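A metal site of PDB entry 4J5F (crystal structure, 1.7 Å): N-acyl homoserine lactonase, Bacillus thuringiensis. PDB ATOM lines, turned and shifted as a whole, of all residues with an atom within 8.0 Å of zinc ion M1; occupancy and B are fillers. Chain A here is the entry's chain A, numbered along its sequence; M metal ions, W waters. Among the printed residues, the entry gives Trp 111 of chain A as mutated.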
ATOM      1  N   CYS A  18      -2.019  14.389 -14.086  1.00  0.00           N
ATOM      2  CA  CYS A  18      -2.843  15.473 -14.628  1.00  0.00           C
ATOM      3  C   CYS A  18      -3.603  16.213 -13.545  1.00  0.00           C
ATOM      4  O   CYS A  18      -4.171  15.611 -12.643  1.00  0.00           O
ATOM      5  CB  CYS A  18      -3.797  14.939 -15.698  1.00  0.00           C
ATOM      6  SG  CYS A  18      -5.098  13.864 -15.070  1.00  0.00           S
ATOM      7  N   LEU A  20      -6.746  18.209 -12.460  1.00  0.00           N
ATOM      8  CA  LEU A  20      -8.143  18.407 -12.779  1.00  0.00           C
ATOM      9  C   LEU A  20      -8.802  19.135 -11.618  1.00  0.00           C
ATOM     10  O   LEU A  20      -8.336  19.040 -10.480  1.00  0.00           O
ATOM     11  CB  LEU A  20      -8.858  17.067 -12.932  1.00  0.00           C
ATOM     12  CG  LEU A  20      -8.393  16.084 -13.989  1.00  0.00           C
ATOM     13  CD1 LEU A  20      -9.419  14.948 -14.073  1.00  0.00           C
ATOM     14  CD2 LEU A  20      -8.287  16.789 -15.322  1.00  0.00           C
ATOM     15  N   LEU A  37      -3.681  14.185 -10.239  1.00  0.00           N
ATOM     16  CA  LEU A  37      -4.195  12.813 -10.285  1.00  0.00           C
ATOM     17  C   LEU A  37      -3.221  11.957 -11.082  1.00  0.00           C
ATOM     18  O   LEU A  37      -2.573  12.446 -12.021  1.00  0.00           O
ATOM     19  CB  LEU A  37      -5.560  12.792 -10.980  1.00  0.00           C
ATOM     20  CG  LEU A  37      -6.737  13.510 -10.312  1.00  0.00           C
ATOM     21  CD1 LEU A  37      -7.988  13.324 -11.100  1.00  0.00           C
ATOM     22  CD2 LEU A  37      -6.918  12.943  -8.914  1.00  0.00           C
ATOM     23  N   PRO A  38      -3.149  10.650 -10.751  1.00  0.00           N
ATOM     24  CA  PRO A  38      -2.268   9.749 -11.499  1.00  0.00           C
ATOM     25  C   PRO A  38      -2.888   9.396 -12.873  1.00  0.00           C
ATOM     26  O   PRO A  38      -4.121   9.266 -12.955  1.00  0.00           O
ATOM     27  CB  PRO A  38      -2.272   8.496 -10.643  1.00  0.00           C
ATOM     28  CG  PRO A  38      -3.620   8.509  -9.965  1.00  0.00           C
ATOM     29  CD  PRO A  38      -3.913   9.949  -9.699  1.00  0.00           C
ATOM     30  N   VAL A  39      -2.044   9.197 -13.885  1.00  0.00           N
ATOM     31  CA  VAL A  39      -2.477   8.606 -15.173  1.00  0.00           C
ATOM     32  C   VAL A  39      -1.749   7.272 -15.197  1.00  0.00           C
ATOM     33  O   VAL A  39      -0.576   7.202 -14.856  1.00  0.00           O
ATOM     34  CB  VAL A  39      -1.982   9.447 -16.339  1.00  0.00           C
ATOM     35  CG1 VAL A  39      -2.226   8.743 -17.732  1.00  0.00           C
ATOM     36  CG2 VAL A  39      -2.674  10.792 -16.275  1.00  0.00           C
ATOM     37  N   TRP A  40      -2.455   6.211 -15.574  1.00  0.00           N
ATOM     38  CA  TRP A  40      -1.905   4.859 -15.502  1.00  0.00           C
ATOM     39  C   TRP A  40      -1.947   4.231 -16.887  1.00  0.00           C
ATOM     40  O   TRP A  40      -2.875   4.506 -17.687  1.00  0.00           O
ATOM     41  CB  TRP A  40      -2.852   3.999 -14.633  1.00  0.00           C
ATOM     42  CG  TRP A  40      -2.893   4.337 -13.149  1.00  0.00           C
ATOM     43  CD1 TRP A  40      -3.907   4.928 -12.452  1.00  0.00           C
ATOM     44  CD2 TRP A  40      -1.863   4.043 -12.189  1.00  0.00           C
ATOM     45  NE1 TRP A  40      -3.561   5.017 -11.106  1.00  0.00           N
ATOM     46  CE2 TRP A  40      -2.317   4.486 -10.928  1.00  0.00           C
ATOM     47  CE3 TRP A  40      -0.593   3.466 -12.288  1.00  0.00           C
ATOM     48  CZ2 TRP A  40      -1.531   4.348  -9.748  1.00  0.00           C
ATOM     49  CZ3 TRP A  40       0.182   3.333 -11.124  1.00  0.00           C
ATOM     50  CH2 TRP A  40      -0.293   3.780  -9.872  1.00  0.00           C
ATOM     51  N   ASP A  54      -3.949   0.760 -22.339  1.00  0.00           N
ATOM     52  CA  ASP A  54      -3.922   2.207 -22.428  1.00  0.00           C
ATOM     53  C   ASP A  54      -2.538   2.693 -22.786  1.00  0.00           C
ATOM     54  O   ASP A  54      -1.609   1.985 -22.627  1.00  0.00           O
ATOM     55  CB  ASP A  54      -4.551   2.884 -21.236  1.00  0.00           C
ATOM     56  CG  ASP A  54      -6.068   2.710 -21.198  1.00  0.00           C
ATOM     57  OD1 ASP A  54      -6.625   2.298 -22.204  1.00  0.00           O
ATOM     58  OD2 ASP A  54      -6.683   2.996 -20.192  1.00  0.00           O
ATOM     59  N   SER A 107      -9.173   1.165 -22.916  1.00  0.00           N
ATOM     60  CA  SER A 107     -10.369   1.211 -22.051  1.00  0.00           C
ATOM     61  C   SER A 107     -11.374   2.163 -22.663  1.00  0.00           C
ATOM     62  O   SER A 107     -12.585   1.887 -22.693  1.00  0.00           O
ATOM     63  CB  SER A 107      -9.988   1.732 -20.673  1.00  0.00           C
ATOM     64  OG  SER A 107      -9.364   3.005 -20.789  1.00  0.00           O
ATOM     65  N   HIS A 108     -10.860   3.312 -23.106  1.00  0.00           N
ATOM     66  CA  HIS A 108     -11.617   4.262 -23.909  1.00  0.00           C
ATOM     67  C   HIS A 108     -10.657   5.233 -24.597  1.00  0.00           C
ATOM     68  O   HIS A 108      -9.446   5.113 -24.421  1.00  0.00           O
ATOM     69  CB  HIS A 108     -12.623   5.019 -23.064  1.00  0.00           C
ATOM     70  CG  HIS A 108     -12.039   5.759 -21.899  1.00  0.00           C
ATOM     71  ND1 HIS A 108     -11.215   5.159 -20.958  1.00  0.00           N
ATOM     72  CD2 HIS A 108     -12.244   7.022 -21.462  1.00  0.00           C
ATOM     73  CE1 HIS A 108     -10.927   6.032 -20.012  1.00  0.00           C
ATOM     74  NE2 HIS A 108     -11.527   7.173 -20.288  1.00  0.00           N
ATOM     75  N   HIS A 110     -10.392   8.673 -24.447  1.00  0.00           N
ATOM     76  CA  HIS A 110     -10.094   9.980 -23.860  1.00  0.00           C
ATOM     77  C   HIS A 110      -8.597  10.251 -23.974  1.00  0.00           C
ATOM     78  O   HIS A 110      -7.795   9.326 -24.044  1.00  0.00           O
ATOM     79  CB  HIS A 110     -10.496  10.063 -22.395  1.00  0.00           C
ATOM     80  CG  HIS A 110     -11.962  10.253 -22.169  1.00  0.00           C
ATOM     81  ND1 HIS A 110     -12.543  10.057 -20.924  1.00  0.00           N
ATOM     82  CD2 HIS A 110     -12.978  10.612 -23.004  1.00  0.00           C
ATOM     83  CE1 HIS A 110     -13.846  10.302 -21.005  1.00  0.00           C
ATOM     84  NE2 HIS A 110     -14.136  10.619 -22.255  1.00  0.00           N
ATOM     85  N   TRP A 111      -8.243  11.542 -23.976  1.00  0.00           N
ATOM     86  CA  TRP A 111      -6.882  12.025 -24.237  1.00  0.00           C
ATOM     87  C   TRP A 111      -5.814  11.407 -23.284  1.00  0.00           C
ATOM     88  O   TRP A 111      -4.656  11.260 -23.679  1.00  0.00           O
ATOM     89  CB  TRP A 111      -6.882  13.577 -24.156  1.00  0.00           C
ATOM     90  CG  TRP A 111      -6.922  13.999 -22.726  1.00  0.00           C
ATOM     91  CD1 TRP A 111      -8.016  14.023 -21.894  1.00  0.00           C
ATOM     92  CD2 TRP A 111      -5.805  14.406 -21.940  1.00  0.00           C
ATOM     93  NE1 TRP A 111      -7.629  14.429 -20.627  1.00  0.00           N
ATOM     94  CE2 TRP A 111      -6.277  14.667 -20.633  1.00  0.00           C
ATOM     95  CE3 TRP A 111      -4.446  14.593 -22.212  1.00  0.00           C
ATOM     96  CZ2 TRP A 111      -5.430  15.095 -19.601  1.00  0.00           C
ATOM     97  CZ3 TRP A 111      -3.605  15.023 -21.189  1.00  0.00           C
ATOM     98  CH2 TRP A 111      -4.100  15.254 -19.898  1.00  0.00           C
ATOM     99  N   ASP A 112      -6.227  11.003 -22.092  1.00  0.00           N
ATOM    100  CA  ASP A 112      -5.258  10.529 -21.083  1.00  0.00           C
ATOM    101  C   ASP A 112      -5.129   8.983 -21.112  1.00  0.00           C
ATOM    102  O   ASP A 112      -4.403   8.398 -20.298  1.00  0.00           O
ATOM    103  CB  ASP A 112      -5.606  11.031 -19.660  1.00  0.00           C
ATOM    104  CG  ASP A 112      -7.030  10.661 -19.230  1.00  0.00           C
ATOM    105  OD1 ASP A 112      -7.983  10.855 -20.054  1.00  0.00           O
ATOM    106  OD2 ASP A 112      -7.253  10.195 -18.073  1.00  0.00           O
ATOM    107  N   HIS A 113      -5.807   8.344 -22.077  1.00  0.00           N
ATOM    108  CA  HIS A 113      -5.825   6.877 -22.189  1.00  0.00           C
ATOM    109  C   HIS A 113      -5.411   6.387 -23.567  1.00  0.00           C
ATOM    110  O   HIS A 113      -4.964   5.254 -23.709  1.00  0.00           O
ATOM    111  CB  HIS A 113      -7.252   6.343 -21.862  1.00  0.00           C
ATOM    112  CG  HIS A 113      -7.661   6.619 -20.448  1.00  0.00           C
ATOM    113  ND1 HIS A 113      -7.457   5.717 -19.421  1.00  0.00           N
ATOM    114  CD2 HIS A 113      -8.184   7.728 -19.868  1.00  0.00           C
ATOM    115  CE1 HIS A 113      -7.844   6.265 -18.275  1.00  0.00           C
ATOM    116  NE2 HIS A 113      -8.277   7.488 -18.519  1.00  0.00           N
ATOM    117  N   HIS A 173     -19.043   6.768 -18.282  1.00  0.00           N
ATOM    118  CA  HIS A 173     -18.016   7.788 -18.199  1.00  0.00           C
ATOM    119  C   HIS A 173     -17.697   8.266 -19.616  1.00  0.00           C
ATOM    120  O   HIS A 173     -17.418   9.467 -19.830  1.00  0.00           O
ATOM    121  CB  HIS A 173     -16.748   7.232 -17.550  1.00  0.00           C
ATOM    122  CG  HIS A 173     -15.539   8.097 -17.732  1.00  0.00           C
ATOM    123  ND1 HIS A 173     -15.378   9.293 -17.071  1.00  0.00           N
ATOM    124  CD2 HIS A 173     -14.432   7.920 -18.485  1.00  0.00           C
ATOM    125  CE1 HIS A 173     -14.226   9.830 -17.417  1.00  0.00           C
ATOM    126  NE2 HIS A 173     -13.620   9.010 -18.252  1.00  0.00           N
ATOM    127  N   HIS A 177     -16.874   2.994 -22.824  1.00  0.00           N
ATOM    128  CA  HIS A 177     -15.886   2.646 -21.813  1.00  0.00           C
ATOM    129  C   HIS A 177     -15.945   1.158 -21.437  1.00  0.00           C
ATOM    130  O   HIS A 177     -17.036   0.536 -21.398  1.00  0.00           O
ATOM    131  CB  HIS A 177     -16.116   3.482 -20.575  1.00  0.00           C
ATOM    132  CG  HIS A 177     -15.070   3.264 -19.526  1.00  0.00           C
ATOM    133  ND1 HIS A 177     -15.126   2.206 -18.632  1.00  0.00           N
ATOM    134  CD2 HIS A 177     -13.909   3.912 -19.268  1.00  0.00           C
ATOM    135  CE1 HIS A 177     -14.077   2.256 -17.841  1.00  0.00           C
ATOM    136  NE2 HIS A 177     -13.320   3.279 -18.199  1.00  0.00           N
ATOM    137  N   ILE A 194     -10.865   1.020 -14.309  1.00  0.00           N
ATOM    138  CA  ILE A 194     -10.465   2.143 -15.118  1.00  0.00           C
ATOM    139  C   ILE A 194     -11.367   3.289 -14.724  1.00  0.00           C
ATOM    140  O   ILE A 194     -11.580   3.493 -13.567  1.00  0.00           O
ATOM    141  CB  ILE A 194     -10.477   1.866 -16.604  1.00  0.00           C
ATOM    142  CG1 ILE A 194      -9.956   0.467 -16.907  1.00  0.00           C
ATOM    143  CG2 ILE A 194      -9.661   2.904 -17.331  1.00  0.00           C
ATOM    144  CD1 ILE A 194      -8.504   0.242 -16.641  1.00  0.00           C
ATOM    145  N   ASP A 195     -11.942   3.989 -15.693  1.00  0.00           N
ATOM    146  CA  ASP A 195     -12.710   5.203 -15.369  1.00  0.00           C
ATOM    147  C   ASP A 195     -14.212   4.966 -15.137  1.00  0.00           C
ATOM    148  O   ASP A 195     -15.008   5.914 -15.102  1.00  0.00           O
ATOM    149  CB  ASP A 195     -12.440   6.312 -16.398  1.00  0.00           C
ATOM    150  CG  ASP A 195     -11.045   6.921 -16.283  1.00  0.00           C
ATOM    151  OD1 ASP A 195     -10.252   6.449 -15.415  1.00  0.00           O
ATOM    152  OD2 ASP A 195     -10.699   7.858 -17.072  1.00  0.00           O
ATOM    153  N   ALA A 196     -14.614   3.699 -14.980  1.00  0.00           N
ATOM    154  CA  ALA A 196     -15.965   3.390 -14.582  1.00  0.00           C
ATOM    155  C   ALA A 196     -16.137   3.817 -13.094  1.00  0.00           C
ATOM    156  O   ALA A 196     -17.264   3.963 -12.598  1.00  0.00           O
ATOM    157  CB  ALA A 196     -16.295   1.898 -14.816  1.00  0.00           C
ATOM    158  N   TYR A 198     -13.529   6.789 -10.937  1.00  0.00           N
ATOM    159  CA  TYR A 198     -12.263   7.466 -10.667  1.00  0.00           C
ATOM    160  C   TYR A 198     -11.656   7.073  -9.320  1.00  0.00           C
ATOM    161  O   TYR A 198     -10.449   6.852  -9.222  1.00  0.00           O
ATOM    162  CB  TYR A 198     -12.396   8.990 -10.628  1.00  0.00           C
ATOM    163  CG  TYR A 198     -12.357   9.687 -11.970  1.00  0.00           C
ATOM    164  CD1 TYR A 198     -12.665   9.003 -13.127  1.00  0.00           C
ATOM    165  CD2 TYR A 198     -12.005  11.009 -12.072  1.00  0.00           C
ATOM    166  CE1 TYR A 198     -12.646   9.651 -14.359  1.00  0.00           C
ATOM    167  CE2 TYR A 198     -11.990  11.665 -13.299  1.00  0.00           C
ATOM    168  CZ  TYR A 198     -12.302  10.971 -14.421  1.00  0.00           C
ATOM    169  OH  TYR A 198     -12.269  11.635 -15.621  1.00  0.00           O
ATOM    170  N   GLY A 238      -9.658   4.239 -11.238  1.00  0.00           N
ATOM    171  CA  GLY A 238      -8.966   4.853 -12.370  1.00  0.00           C
ATOM    172  C   GLY A 238      -8.047   6.027 -12.080  1.00  0.00           C
ATOM    173  O   GLY A 238      -7.010   6.202 -12.751  1.00  0.00           O
ATOM    174  N   HIS A 239      -8.431   6.865 -11.116  1.00  0.00           N
ATOM    175  CA  HIS A 239      -7.728   8.116 -10.913  1.00  0.00           C
ATOM    176  C   HIS A 239      -7.790   8.471  -9.412  1.00  0.00           C
ATOM    177  O   HIS A 239      -8.369   9.492  -9.032  1.00  0.00           O
ATOM    178  CB  HIS A 239      -8.371   9.218 -11.793  1.00  0.00           C
ATOM    179  CG  HIS A 239      -8.073   9.114 -13.282  1.00  0.00           C
ATOM    180  ND1 HIS A 239      -6.796   9.194 -13.788  1.00  0.00           N
ATOM    181  CD2 HIS A 239      -8.895   9.019 -14.368  1.00  0.00           C
ATOM    182  CE1 HIS A 239      -6.826   9.136 -15.111  1.00  0.00           C
ATOM    183  NE2 HIS A 239      -8.087   9.046 -15.490  1.00  0.00           N
HETATM  184 ZN    ZN M   1      -9.009   8.832 -17.304  1.00  0.00          ZN
HETATM  185 ZN    ZN M   2     -11.863   9.042 -19.236  1.00  0.00          ZN
HETATM  186  O   HOH W   1     -10.698  10.628 -17.206  1.00  0.00           O
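A ring nitrogen (ND1) of His 113 lies within hydrogen-bond range of the side-chain carboxylate of Asp 54 (2.9 Å).
N of Asp 195 sits at hydrogen-bond distance from NE2 of His 177, at 2.9 Å.
N of His 239 sits at hydrogen-bond distance from O of Tyr 198 (2.8 Å).
A ring nitrogen (ND1) of His 239 is in hydrogen-bond range of the backbone carbonyl oxygen (O) of Pro 38, 2.8 Å away.
Within 4 Å of zinc ion M1: Asp 112, His 113, Asp 195 and His 239.
The nearest printed residue that does not touch zinc ion M1 is His 108 (4.2 Å).
Zinc ion M1 is bound by NE2 of His 113 (2.0 Å), OD2 of Asp 195 (2.0 Å), NE2 of His 239 (2.0 Å), OD2 of Asp 112 (2.4 Å) and water W1 (2.5 Å).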
